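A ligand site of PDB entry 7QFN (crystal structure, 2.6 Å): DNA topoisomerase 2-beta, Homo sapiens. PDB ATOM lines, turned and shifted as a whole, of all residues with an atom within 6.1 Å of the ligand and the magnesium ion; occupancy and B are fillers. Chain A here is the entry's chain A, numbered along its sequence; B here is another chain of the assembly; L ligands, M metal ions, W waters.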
ATOM      1  N   GLU A  62      -4.531  -6.110  23.959  1.00  0.00           N
ATOM      2  CA  GLU A  62      -5.126  -4.810  24.231  1.00  0.00           C
ATOM      3  C   GLU A  62      -5.615  -4.747  25.673  1.00  0.00           C
ATOM      4  O   GLU A  62      -5.395  -3.723  26.362  1.00  0.00           O
ATOM      5  CB  GLU A  62      -6.280  -4.543  23.256  1.00  0.00           C
ATOM      6  CG  GLU A  62      -5.881  -3.696  22.055  1.00  0.00           C
ATOM      7  CD  GLU A  62      -4.994  -2.521  22.443  1.00  0.00           C
ATOM      8  OE1 GLU A  62      -4.014  -2.281  21.683  1.00  0.00           O
ATOM      9  OE2 GLU A  62      -5.246  -1.871  23.557  1.00  0.00           O
ATOM     10  N   ILE A  63      -6.294  -5.820  26.109  1.00  0.00           N
ATOM     11  CA  ILE A  63      -6.953  -5.884  27.403  1.00  0.00           C
ATOM     12  C   ILE A  63      -5.923  -6.069  28.511  1.00  0.00           C
ATOM     13  O   ILE A  63      -6.016  -5.467  29.577  1.00  0.00           O
ATOM     14  CB  ILE A  63      -7.990  -7.043  27.471  1.00  0.00           C
ATOM     15  CG1 ILE A  63      -9.087  -6.882  26.428  1.00  0.00           C
ATOM     16  CG2 ILE A  63      -8.561  -7.168  28.883  1.00  0.00           C
ATOM     17  CD1 ILE A  63      -9.593  -5.453  26.251  1.00  0.00           C
ATOM     18  N   VAL A  65      -2.806  -5.239  28.292  1.00  0.00           N
ATOM     19  CA  VAL A  65      -2.032  -4.007  28.433  1.00  0.00           C
ATOM     20  C   VAL A  65      -2.817  -2.946  29.216  1.00  0.00           C
ATOM     21  O   VAL A  65      -2.205  -2.110  29.900  1.00  0.00           O
ATOM     22  CB  VAL A  65      -1.504  -3.494  27.067  1.00  0.00           C
ATOM     23  CG1 VAL A  65      -0.874  -2.105  27.159  1.00  0.00           C
ATOM     24  CG2 VAL A  65      -0.494  -4.483  26.474  1.00  0.00           C
ATOM     25  N   ASN A  66      -4.169  -2.991  29.123  1.00  0.00           N
ATOM     26  CA  ASN A  66      -5.008  -2.035  29.847  1.00  0.00           C
ATOM     27  C   ASN A  66      -4.857  -2.217  31.382  1.00  0.00           C
ATOM     28  O   ASN A  66      -4.831  -1.238  32.160  1.00  0.00           O
ATOM     29  CB  ASN A  66      -6.472  -2.136  29.400  1.00  0.00           C
ATOM     30  CG  ASN A  66      -6.909  -1.380  28.164  1.00  0.00           C
ATOM     31  OD1 ASN A  66      -6.200  -0.517  27.638  1.00  0.00           O
ATOM     32  ND2 ASN A  66      -8.094  -1.749  27.674  1.00  0.00           N
ATOM     33  N   ALA A  67      -4.800  -3.479  31.850  1.00  0.00           N
ATOM     34  CA  ALA A  67      -4.528  -3.814  33.256  1.00  0.00           C
ATOM     35  C   ALA A  67      -3.177  -3.261  33.679  1.00  0.00           C
ATOM     36  O   ALA A  67      -3.120  -2.537  34.673  1.00  0.00           O
ATOM     37  CB  ALA A  67      -4.497  -5.323  33.482  1.00  0.00           C
ATOM     38  N   ASP A  69      -1.576  -0.859  32.479  1.00  0.00           N
ATOM     39  CA  ASP A  69      -1.580   0.596  32.484  1.00  0.00           C
ATOM     40  C   ASP A  69      -2.173   1.111  33.788  1.00  0.00           C
ATOM     41  O   ASP A  69      -1.810   2.222  34.183  1.00  0.00           O
ATOM     42  CB  ASP A  69      -2.423   1.179  31.349  1.00  0.00           C
ATOM     43  CG  ASP A  69      -1.856   1.122  29.943  1.00  0.00           C
ATOM     44  OD1 ASP A  69      -0.632   0.801  29.798  1.00  0.00           O
ATOM     45  OD2 ASP A  69      -2.641   1.411  28.990  1.00  0.00           O
ATOM     46  N   ASN A  70      -3.061   0.304  34.416  1.00  0.00           N
ATOM     47  CA  ASN A  70      -3.776   0.796  35.602  1.00  0.00           C
ATOM     48  C   ASN A  70      -2.820   0.947  36.783  1.00  0.00           C
ATOM     49  O   ASN A  70      -3.074   1.694  37.711  1.00  0.00           O
ATOM     50  CB  ASN A  70      -4.981  -0.051  35.995  1.00  0.00           C
ATOM     51  CG  ASN A  70      -5.789   0.612  37.080  1.00  0.00           C
ATOM     52  OD1 ASN A  70      -6.407   1.649  36.795  1.00  0.00           O
ATOM     53  ND2 ASN A  70      -5.774   0.051  38.276  1.00  0.00           N
ATOM     54  N   ARG A  73      -1.495   4.135  36.514  1.00  0.00           N
ATOM     55  CA  ARG A  73      -2.586   5.014  36.953  1.00  0.00           C
ATOM     56  C   ARG A  73      -2.740   5.007  38.467  1.00  0.00           C
ATOM     57  O   ARG A  73      -3.043   6.025  39.081  1.00  0.00           O
ATOM     58  CB  ARG A  73      -3.876   4.533  36.292  1.00  0.00           C
ATOM     59  CG  ARG A  73      -5.120   5.250  36.774  1.00  0.00           C
ATOM     60  CD  ARG A  73      -6.329   4.963  35.919  1.00  0.00           C
ATOM     61  NE  ARG A  73      -7.542   5.425  36.618  1.00  0.00           N
ATOM     62  CZ  ARG A  73      -8.464   4.634  37.181  1.00  0.00           C
ATOM     63  NH1 ARG A  73      -8.375   3.306  37.137  1.00  0.00           N
ATOM     64  NH2 ARG A  73      -9.482   5.202  37.819  1.00  0.00           N
ATOM     65  N   ASN A  95      -7.786  -7.058  37.386  1.00  0.00           N
ATOM     66  CA  ASN A  95      -6.816  -6.301  38.148  1.00  0.00           C
ATOM     67  C   ASN A  95      -7.528  -5.609  39.326  1.00  0.00           C
ATOM     68  O   ASN A  95      -8.772  -5.542  39.361  1.00  0.00           O
ATOM     69  CB  ASN A  95      -6.067  -5.341  37.224  1.00  0.00           C
ATOM     70  CG  ASN A  95      -6.890  -4.122  36.849  1.00  0.00           C
ATOM     71  OD1 ASN A  95      -7.663  -4.223  35.896  1.00  0.00           O
ATOM     72  ND2 ASN A  95      -6.772  -3.005  37.574  1.00  0.00           N
ATOM     73  N   LYS A  98      -7.202   0.942  41.646  1.00  0.00           N
ATOM     74  CA  LYS A  98      -8.353   1.787  41.537  1.00  0.00           C
ATOM     75  C   LYS A  98      -9.200   1.294  40.347  1.00  0.00           C
ATOM     76  O   LYS A  98      -8.663   0.980  39.271  1.00  0.00           O
ATOM     77  CB  LYS A  98      -7.906   3.259  41.508  1.00  0.00           C
ATOM     78  CG  LYS A  98      -9.040   4.223  41.809  1.00  0.00           C
ATOM     79  CD  LYS A  98      -8.725   5.683  41.723  1.00  0.00           C
ATOM     80  CE  LYS A  98      -9.953   6.528  42.015  1.00  0.00           C
ATOM     81  NZ  LYS A  98     -10.589   6.206  43.324  1.00  0.00           N
ATOM     82  N   GLY A  99     -10.514   1.198  40.594  1.00  0.00           N
ATOM     83  CA  GLY A  99     -11.470   0.799  39.574  1.00  0.00           C
ATOM     84  C   GLY A  99     -11.810   1.979  38.652  1.00  0.00           C
ATOM     85  O   GLY A  99     -11.044   2.925  38.519  1.00  0.00           O
ATOM     86  N   ILE A 100     -12.977   1.880  37.996  1.00  0.00           N
ATOM     87  CA  ILE A 100     -13.447   2.909  37.083  1.00  0.00           C
ATOM     88  C   ILE A 100     -14.693   3.557  37.680  1.00  0.00           C
ATOM     89  O   ILE A 100     -15.680   2.908  38.017  1.00  0.00           O
ATOM     90  CB  ILE A 100     -13.717   2.350  35.676  1.00  0.00           C
ATOM     91  CG1 ILE A 100     -12.459   1.733  35.046  1.00  0.00           C
ATOM     92  CG2 ILE A 100     -14.281   3.442  34.779  1.00  0.00           C
ATOM     93  CD1 ILE A 100     -12.778   0.656  34.082  1.00  0.00           C
ATOM     94  N   ILE A 116     -16.456   4.077  27.998  1.00  0.00           N
ATOM     95  CA  ILE A 116     -15.087   3.794  27.610  1.00  0.00           C
ATOM     96  C   ILE A 116     -14.887   2.377  27.090  1.00  0.00           C
ATOM     97  O   ILE A 116     -13.840   2.103  26.457  1.00  0.00           O
ATOM     98  CB  ILE A 116     -14.095   4.128  28.738  1.00  0.00           C
ATOM     99  CG1 ILE A 116     -14.284   3.249  29.962  1.00  0.00           C
ATOM    100  CG2 ILE A 116     -14.153   5.624  29.077  1.00  0.00           C
ATOM    101  CD1 ILE A 116     -13.513   3.796  31.144  1.00  0.00           C
ATOM    102  N   PHE A 117     -15.862   1.486  27.331  1.00  0.00           N
ATOM    103  CA  PHE A 117     -15.807   0.117  26.816  1.00  0.00           C
ATOM    104  C   PHE A 117     -16.797  -0.136  25.675  1.00  0.00           C
ATOM    105  O   PHE A 117     -16.717  -1.194  25.053  1.00  0.00           O
ATOM    106  CB  PHE A 117     -16.036  -0.877  27.939  1.00  0.00           C
ATOM    107  CG  PHE A 117     -14.784  -1.129  28.732  1.00  0.00           C
ATOM    108  CD1 PHE A 117     -13.838  -2.041  28.271  1.00  0.00           C
ATOM    109  CD2 PHE A 117     -14.519  -0.425  29.902  1.00  0.00           C
ATOM    110  CE1 PHE A 117     -12.642  -2.220  28.960  1.00  0.00           C
ATOM    111  CE2 PHE A 117     -13.335  -0.605  30.583  1.00  0.00           C
ATOM    112  CZ  PHE A 117     -12.400  -1.518  30.114  1.00  0.00           C
ATOM    113  N   THR A 122     -12.724   6.701  22.813  1.00  0.00           N
ATOM    114  CA  THR A 122     -12.912   6.931  24.245  1.00  0.00           C
ATOM    115  C   THR A 122     -11.678   6.435  24.999  1.00  0.00           C
ATOM    116  O   THR A 122     -11.295   5.261  24.905  1.00  0.00           O
ATOM    117  CB  THR A 122     -14.181   6.262  24.807  1.00  0.00           C
ATOM    118  OG1 THR A 122     -14.174   4.834  24.609  1.00  0.00           O
ATOM    119  CG2 THR A 122     -15.463   6.867  24.222  1.00  0.00           C
ATOM    120  N   SER A 123     -11.072   7.382  25.751  1.00  0.00           N
ATOM    121  CA  SER A 123      -9.833   7.147  26.485  1.00  0.00           C
ATOM    122  C   SER A 123      -9.678   8.183  27.593  1.00  0.00           C
ATOM    123  O   SER A 123     -10.022   9.366  27.465  1.00  0.00           O
ATOM    124  CB  SER A 123      -8.591   7.115  25.533  1.00  0.00           C
ATOM    125  OG  SER A 123      -7.317   7.043  26.195  1.00  0.00           O
ATOM    126  N   SER A 124      -9.076   7.690  28.678  1.00  0.00           N
ATOM    127  CA  SER A 124      -8.538   8.565  29.689  1.00  0.00           C
ATOM    128  C   SER A 124      -7.123   9.039  29.329  1.00  0.00           C
ATOM    129  O   SER A 124      -6.473   9.660  30.125  1.00  0.00           O
ATOM    130  CB  SER A 124      -8.565   7.894  31.049  1.00  0.00           C
ATOM    131  OG  SER A 124      -7.448   7.035  31.134  1.00  0.00           O
ATOM    132  N   ASN A 125      -6.615   8.781  28.124  1.00  0.00           N
ATOM    133  CA  ASN A 125      -5.217   9.124  27.833  1.00  0.00           C
ATOM    134  C   ASN A 125      -5.159  10.093  26.661  1.00  0.00           C
ATOM    135  O   ASN A 125      -4.188  10.031  25.934  1.00  0.00           O
ATOM    136  CB  ASN A 125      -4.354   7.905  27.448  1.00  0.00           C
ATOM    137  CG  ASN A 125      -4.447   6.719  28.400  1.00  0.00           C
ATOM    138  OD1 ASN A 125      -3.860   6.777  29.479  1.00  0.00           O
ATOM    139  ND2 ASN A 125      -5.118   5.653  28.009  1.00  0.00           N
ATOM    140  N   GLY A 135       0.697   2.296  27.905  1.00  0.00           N
ATOM    141  CA  GLY A 135       0.496   1.784  26.564  1.00  0.00           C
ATOM    142  C   GLY A 135      -0.673   2.426  25.834  1.00  0.00           C
ATOM    143  O   GLY A 135      -0.608   2.582  24.617  1.00  0.00           O
ATOM    144  N   GLY A 136      -1.757   2.779  26.574  1.00  0.00           N
ATOM    145  CA  GLY A 136      -2.962   3.361  26.005  1.00  0.00           C
ATOM    146  C   GLY A 136      -2.708   4.799  25.534  1.00  0.00           C
ATOM    147  O   GLY A 136      -1.916   5.529  26.147  1.00  0.00           O
ATOM    148  N   ARG A 137      -3.392   5.175  24.448  1.00  0.00           N
ATOM    149  CA  ARG A 137      -3.110   6.442  23.775  1.00  0.00           C
ATOM    150  C   ARG A 137      -4.213   6.733  22.759  1.00  0.00           C
ATOM    151  O   ARG A 137      -4.709   7.855  22.723  1.00  0.00           O
ATOM    152  CB  ARG A 137      -1.700   6.379  23.159  1.00  0.00           C
ATOM    153  CG  ARG A 137      -1.482   7.209  21.911  1.00  0.00           C
ATOM    154  CD  ARG A 137      -0.382   6.615  21.044  1.00  0.00           C
ATOM    155  NE  ARG A 137      -0.325   7.179  19.692  1.00  0.00           N
ATOM    156  CZ  ARG A 137       0.169   8.370  19.409  1.00  0.00           C
ATOM    157  NH1 ARG A 137       0.100   8.875  18.174  1.00  0.00           N
ATOM    158  NH2 ARG A 137       0.696   9.073  20.398  1.00  0.00           N
ATOM    159  N   ASN A 138      -4.633   5.701  21.985  1.00  0.00           N
ATOM    160  CA  ASN A 138      -5.508   5.950  20.857  1.00  0.00           C
ATOM    161  C   ASN A 138      -6.976   5.682  21.189  1.00  0.00           C
ATOM    162  O   ASN A 138      -7.860   6.117  20.474  1.00  0.00           O
ATOM    163  CB  ASN A 138      -5.127   5.207  19.580  1.00  0.00           C
ATOM    164  CG  ASN A 138      -3.672   5.353  19.183  1.00  0.00           C
ATOM    165  OD1 ASN A 138      -3.170   6.444  18.901  1.00  0.00           O
ATOM    166  ND2 ASN A 138      -2.972   4.237  19.170  1.00  0.00           N
ATOM    167  N   GLY A 139      -7.300   5.030  22.278  1.00  0.00           N
ATOM    168  CA  GLY A 139      -8.707   5.090  22.690  1.00  0.00           C
ATOM    169  C   GLY A 139      -9.639   4.194  21.854  1.00  0.00           C
ATOM    170  O   GLY A 139     -10.847   4.403  21.817  1.00  0.00           O
ATOM    171  N   TYR A 140      -9.012   3.251  21.148  1.00  0.00           N
ATOM    172  CA  TYR A 140      -9.586   2.039  20.561  1.00  0.00           C
ATOM    173  C   TYR A 140      -8.905   0.925  21.316  1.00  0.00           C
ATOM    174  O   TYR A 140      -7.779   1.067  21.774  1.00  0.00           O
ATOM    175  CB  TYR A 140      -9.065   1.758  19.141  1.00  0.00           C
ATOM    176  CG  TYR A 140      -9.427   2.691  17.997  1.00  0.00           C
ATOM    177  CD1 TYR A 140      -8.619   3.756  17.599  1.00  0.00           C
ATOM    178  CD2 TYR A 140     -10.569   2.452  17.250  1.00  0.00           C
ATOM    179  CE1 TYR A 140      -8.977   4.591  16.539  1.00  0.00           C
ATOM    180  CE2 TYR A 140     -10.938   3.266  16.183  1.00  0.00           C
ATOM    181  CZ  TYR A 140     -10.144   4.340  15.817  1.00  0.00           C
ATOM    182  OH  TYR A 140     -10.602   5.086  14.738  1.00  0.00           O
ATOM    183  N   GLY A 141      -9.438  -0.253  21.392  1.00  0.00           N
ATOM    184  CA  GLY A 141      -8.525  -1.189  22.047  1.00  0.00           C
ATOM    185  C   GLY A 141      -9.368  -2.221  22.766  1.00  0.00           C
ATOM    186  O   GLY A 141      -9.554  -3.329  22.277  1.00  0.00           O
ATOM    187  N   ALA A 142      -9.963  -1.711  23.837  1.00  0.00           N
ATOM    188  CA  ALA A 142     -11.109  -2.288  24.496  1.00  0.00           C
ATOM    189  C   ALA A 142     -12.266  -2.382  23.513  1.00  0.00           C
ATOM    190  O   ALA A 142     -12.929  -3.403  23.405  1.00  0.00           O
ATOM    191  CB  ALA A 142     -11.440  -1.442  25.700  1.00  0.00           C
ATOM    192  N   LYS A 143     -12.571  -1.305  22.791  1.00  0.00           N
ATOM    193  CA  LYS A 143     -13.770  -1.410  21.959  1.00  0.00           C
ATOM    194  C   LYS A 143     -13.541  -2.483  20.873  1.00  0.00           C
ATOM    195  O   LYS A 143     -14.449  -3.276  20.640  1.00  0.00           O
ATOM    196  CB  LYS A 143     -14.209  -0.063  21.345  1.00  0.00           C
ATOM    197  CG  LYS A 143     -15.032   0.847  22.242  1.00  0.00           C
ATOM    198  CD  LYS A 143     -14.259   1.434  23.402  1.00  0.00           C
ATOM    199  CE  LYS A 143     -13.068   2.301  23.051  1.00  0.00           C
ATOM    200  NZ  LYS A 143     -12.342   2.664  24.299  1.00  0.00           N
ATOM    201  N   THR A 156     -16.475  -3.419  37.038  1.00  0.00           N
ATOM    202  CA  THR A 156     -15.521  -2.554  37.708  1.00  0.00           C
ATOM    203  C   THR A 156     -16.170  -2.035  38.981  1.00  0.00           C
ATOM    204  O   THR A 156     -17.399  -1.996  39.086  1.00  0.00           O
ATOM    205  CB  THR A 156     -14.994  -1.473  36.740  1.00  0.00           C
ATOM    206  OG1 THR A 156     -13.895  -0.906  37.454  1.00  0.00           O
ATOM    207  CG2 THR A 156     -16.022  -0.432  36.337  1.00  0.00           C
ATOM    208  N   THR A 190     -11.034  -4.262  38.467  1.00  0.00           N
ATOM    209  CA  THR A 190     -11.662  -4.247  37.148  1.00  0.00           C
ATOM    210  C   THR A 190     -11.456  -5.645  36.555  1.00  0.00           C
ATOM    211  O   THR A 190     -10.351  -6.212  36.705  1.00  0.00           O
ATOM    212  CB  THR A 190     -11.122  -3.164  36.199  1.00  0.00           C
ATOM    213  OG1 THR A 190     -11.070  -1.845  36.767  1.00  0.00           O
ATOM    214  CG2 THR A 190     -11.936  -3.133  34.924  1.00  0.00           C
ATOM    215  N   ILE A 192     -12.367  -7.979  33.046  1.00  0.00           N
ATOM    216  CA  ILE A 192     -12.830  -7.961  31.676  1.00  0.00           C
ATOM    217  C   ILE A 192     -12.896  -9.409  31.247  1.00  0.00           C
ATOM    218  O   ILE A 192     -11.878 -10.105  31.314  1.00  0.00           O
ATOM    219  CB  ILE A 192     -11.884  -7.174  30.752  1.00  0.00           C
ATOM    220  CG1 ILE A 192     -11.478  -5.786  31.283  1.00  0.00           C
ATOM    221  CG2 ILE A 192     -12.503  -7.129  29.380  1.00  0.00           C
ATOM    222  CD1 ILE A 192     -12.560  -4.711  31.418  1.00  0.00           C
ATOM    223  N   LYS A 353       1.913  -3.480  16.918  1.00  0.00           N
ATOM    224  CA  LYS A 353       2.889  -2.693  17.668  1.00  0.00           C
ATOM    225  C   LYS A 353       4.256  -3.367  17.863  1.00  0.00           C
ATOM    226  O   LYS A 353       5.068  -2.874  18.643  1.00  0.00           O
ATOM    227  CB  LYS A 353       2.268  -2.340  19.023  1.00  0.00           C
ATOM    228  CG  LYS A 353       1.126  -1.343  18.968  1.00  0.00           C
ATOM    229  CD  LYS A 353       0.255  -1.295  20.217  1.00  0.00           C
ATOM    230  CE  LYS A 353      -1.102  -0.681  19.940  1.00  0.00           C
ATOM    231  NZ  LYS A 353      -1.726  -0.061  21.125  1.00  0.00           N
ATOM    232  N   TYR B   9     -11.843  11.328  31.433  1.00  0.00           N
ATOM    233  CA  TYR B   9     -12.491  10.336  30.599  1.00  0.00           C
ATOM    234  C   TYR B   9     -13.157  11.094  29.446  1.00  0.00           C
ATOM    235  O   TYR B   9     -14.140  11.788  29.677  1.00  0.00           O
ATOM    236  CB  TYR B   9     -13.468   9.516  31.458  1.00  0.00           C
ATOM    237  CG  TYR B   9     -12.818   8.563  32.437  1.00  0.00           C
ATOM    238  CD1 TYR B   9     -12.182   7.405  32.011  1.00  0.00           C
ATOM    239  CD2 TYR B   9     -12.741   8.854  33.787  1.00  0.00           C
ATOM    240  CE1 TYR B   9     -11.548   6.550  32.898  1.00  0.00           C
ATOM    241  CE2 TYR B   9     -12.085   8.021  34.690  1.00  0.00           C
ATOM    242  CZ  TYR B   9     -11.481   6.850  34.250  1.00  0.00           C
ATOM    243  OH  TYR B   9     -10.819   5.988  35.172  1.00  0.00           O
HETATM  244  P1  LIG L   1      -6.630   3.205  25.541  1.00  0.00           P
HETATM  245  O1  LIG L   1      -5.921   2.921  24.197  1.00  0.00           O
HETATM  246  O2  LIG L   1      -6.667   4.606  26.052  1.00  0.00           O
HETATM  247  O3  LIG L   1      -6.132   2.200  26.509  1.00  0.00           O
HETATM  248  P2  LIG L   1      -8.727   1.413  25.561  1.00  0.00           P
HETATM  249  O4  LIG L   1      -9.863   1.172  24.630  1.00  0.00           O
HETATM  250  O5  LIG L   1      -7.484   0.555  25.613  1.00  0.00           O
HETATM  251  O6  LIG L   1      -8.198   2.931  25.444  1.00  0.00           O
HETATM  252  O7  LIG L   1      -9.396   1.512  26.985  1.00  0.00           O
HETATM  253  C1  LIG L   1     -10.403   2.583  27.086  1.00  0.00           C
HETATM  254  C2  LIG L   1     -10.235   3.322  28.404  1.00  0.00           C
HETATM  255  O8  LIG L   1     -10.868   2.585  29.492  1.00  0.00           O
HETATM  256  C3  LIG L   1      -8.771   3.533  28.838  1.00  0.00           C
HETATM  257  O9  LIG L   1      -8.225   4.775  28.370  1.00  0.00           O
HETATM  258  C4  LIG L   1      -8.847   3.492  30.370  1.00  0.00           C
HETATM  259  O10 LIG L   1      -9.054   4.807  30.813  1.00  0.00           O
HETATM  260  C5  LIG L   1     -10.059   2.603  30.654  1.00  0.00           C
HETATM  261  N1  LIG L   1      -9.657   1.257  31.020  1.00  0.00           N
HETATM  262  C6  LIG L   1      -9.479   0.174  30.198  1.00  0.00           C
HETATM  263  N2  LIG L   1      -9.089  -0.916  30.823  1.00  0.00           N
HETATM  264  C7  LIG L   1      -8.937  -0.510  32.135  1.00  0.00           C
HETATM  265  C8  LIG L   1      -8.509  -1.197  33.299  1.00  0.00           C
HETATM  266  N3  LIG L   1      -8.172  -2.483  33.288  1.00  0.00           N
HETATM  267  N4  LIG L   1      -8.528  -0.506  34.470  1.00  0.00           N
HETATM  268  C9  LIG L   1      -8.890   0.778  34.455  1.00  0.00           C
HETATM  269  N5  LIG L   1      -9.316   1.518  33.431  1.00  0.00           N
HETATM  270  C10 LIG L   1      -9.292   0.818  32.280  1.00  0.00           C
HETATM  271 MG    MG M   1      -5.591  -0.017  25.718  1.00  0.00          MG
HETATM  272  O   HOH W   1      -9.302  -3.529  29.330  1.00  0.00           O
HETATM  273  O   HOH W   2      -8.028  -4.959  31.582  1.00  0.00           O
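Residues that only touch the magnesium ion: Glu 62.
Of the 32 residues printed, 2 come within 4 Å of the magnesium ion.
The nearest printed residue that does not touch the magnesium ion is Gly 136 (4.3 Å).
O of Lys 98 sits at hydrogen-bond distance from NH1 of Arg 73.
The side-chain carboxylate of Glu 62 is in salt-bridge range of the side-chain amino group of Lys 353 (3.2 Å).
The side-chain amino group (NZ) of Lys 143 lies within hydrogen-bond range of the side-chain hydroxyl (OG1) of Thr 122, at 2.9 Å.
The side-chain amino group (NZ) of Lys 143 lies within hydrogen-bond range of the backbone carbonyl oxygen (O) of Ile 116 (2.7 Å).
The guanidinium group of Arg 73 lies within hydrogen-bond range of the backbone carbonyl oxygen of Gly 99 (2.8 Å).
The side-chain amide oxygen (OD1) of Asn 138 sits at hydrogen-bond distance from the guanidinium group (NE) of Arg 137 (3.0 Å).
The backbone NH (N) of Gly 136 lies within hydrogen-bond range of the side-chain carboxylate (OD2) of Asp 69, at 2.9 Å.
The backbone carbonyl oxygen of Ile 116 lies close to the side-chain hydroxyl of Thr 122 (3.3 Å).
Water W2 bridges O of Ile 63 (2.9 Å) and N3 of the ligand (3.0 Å).
Water W1 bridges ND2 of Asn 66 (2.7 Å) and N2 of the ligand (3.0 Å).
The magnesium ion is bound by O5 of the ligand (2.0 Å), OD1 of Asn 66 (2.1 Å) and O3 of the ligand (2.4 Å).
The magnesium ion has three donor atoms within binding distance.
N of Ala 142 sits at hydrogen-bond distance from O4 of the ligand (3.0 Å).
ND2 of Asn 125 sits at hydrogen-bond distance from O2 of the ligand, at 2.7 Å.
N of Gly 139 sits at hydrogen-bond distance from O1 of the ligand (3.2 Å).
O10 of the ligand lies within hydrogen-bond range of OG of Ser 124, at 2.8 Å.
O1 of the ligand is in hydrogen-bond range of N of Arg 137 (3.4 Å).
The backbone NH of Ser 124 is in hydrogen-bond range of an oxygen (O9) of the ligand.
The side-chain hydroxyl of Ser 123 sits at hydrogen-bond distance from an oxygen (O2) of the ligand (2.5 Å).
The side-chain amino group of Lys 143 lies within salt-bridge range of an oxygen (O4) of the ligand.
OD1 of Asn 95 is in hydrogen-bond range of N3 of the ligand (3.2 Å).
Glu 62 touches the ligand (OE2 to O5, 3.9 Å).
N of Ala 67 touches N3 of the ligand, 3.8 Å away.
OD1 of Asn 70 touches C9 of the ligand, 3.5 Å away.
Arg 73 touches the ligand (NH1 to C9, 3.7 Å).
Ile 100 touches the ligand (CG1 to N5, 3.5 Å).
CD1 of Ile 116 touches O8 of the ligand, at 3.3 Å.
CZ of Phe 117 touches C6 of the ligand, at 3.4 Å.
Thr 122 touches the ligand (O to C1, 3.6 Å).
CA of Gly 136 touches O3 of the ligand (3.4 Å).
N of Asn 138 touches O1 of the ligand (3.8 Å).
Tyr 140 touches the ligand.
Gly 141 touches the ligand.
Thr 190 touches the ligand.
Tyr 9 of chain B touches the ligand (CE1 to O10, 3.7 Å).
Hydrophobic or aromatic side chains within 4 Å of the ligand: Ile 100, Ile 116, Phe 117, Ala 142 and Tyr 9 of chain B.
Within 4 Å of the ligand: Glu 62, Asn 66, Ala 67, Asn 70, Arg 73, Asn 95, Ile 100, Ile 116, Phe 117, Thr 122, Ser 123, Ser 124, Asn 125, Gly 136, Arg 137, Asn 138, Gly 139, Tyr 140, Gly 141, Ala 142, Lys 143, Thr 190 and Tyr 9 of chain B.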
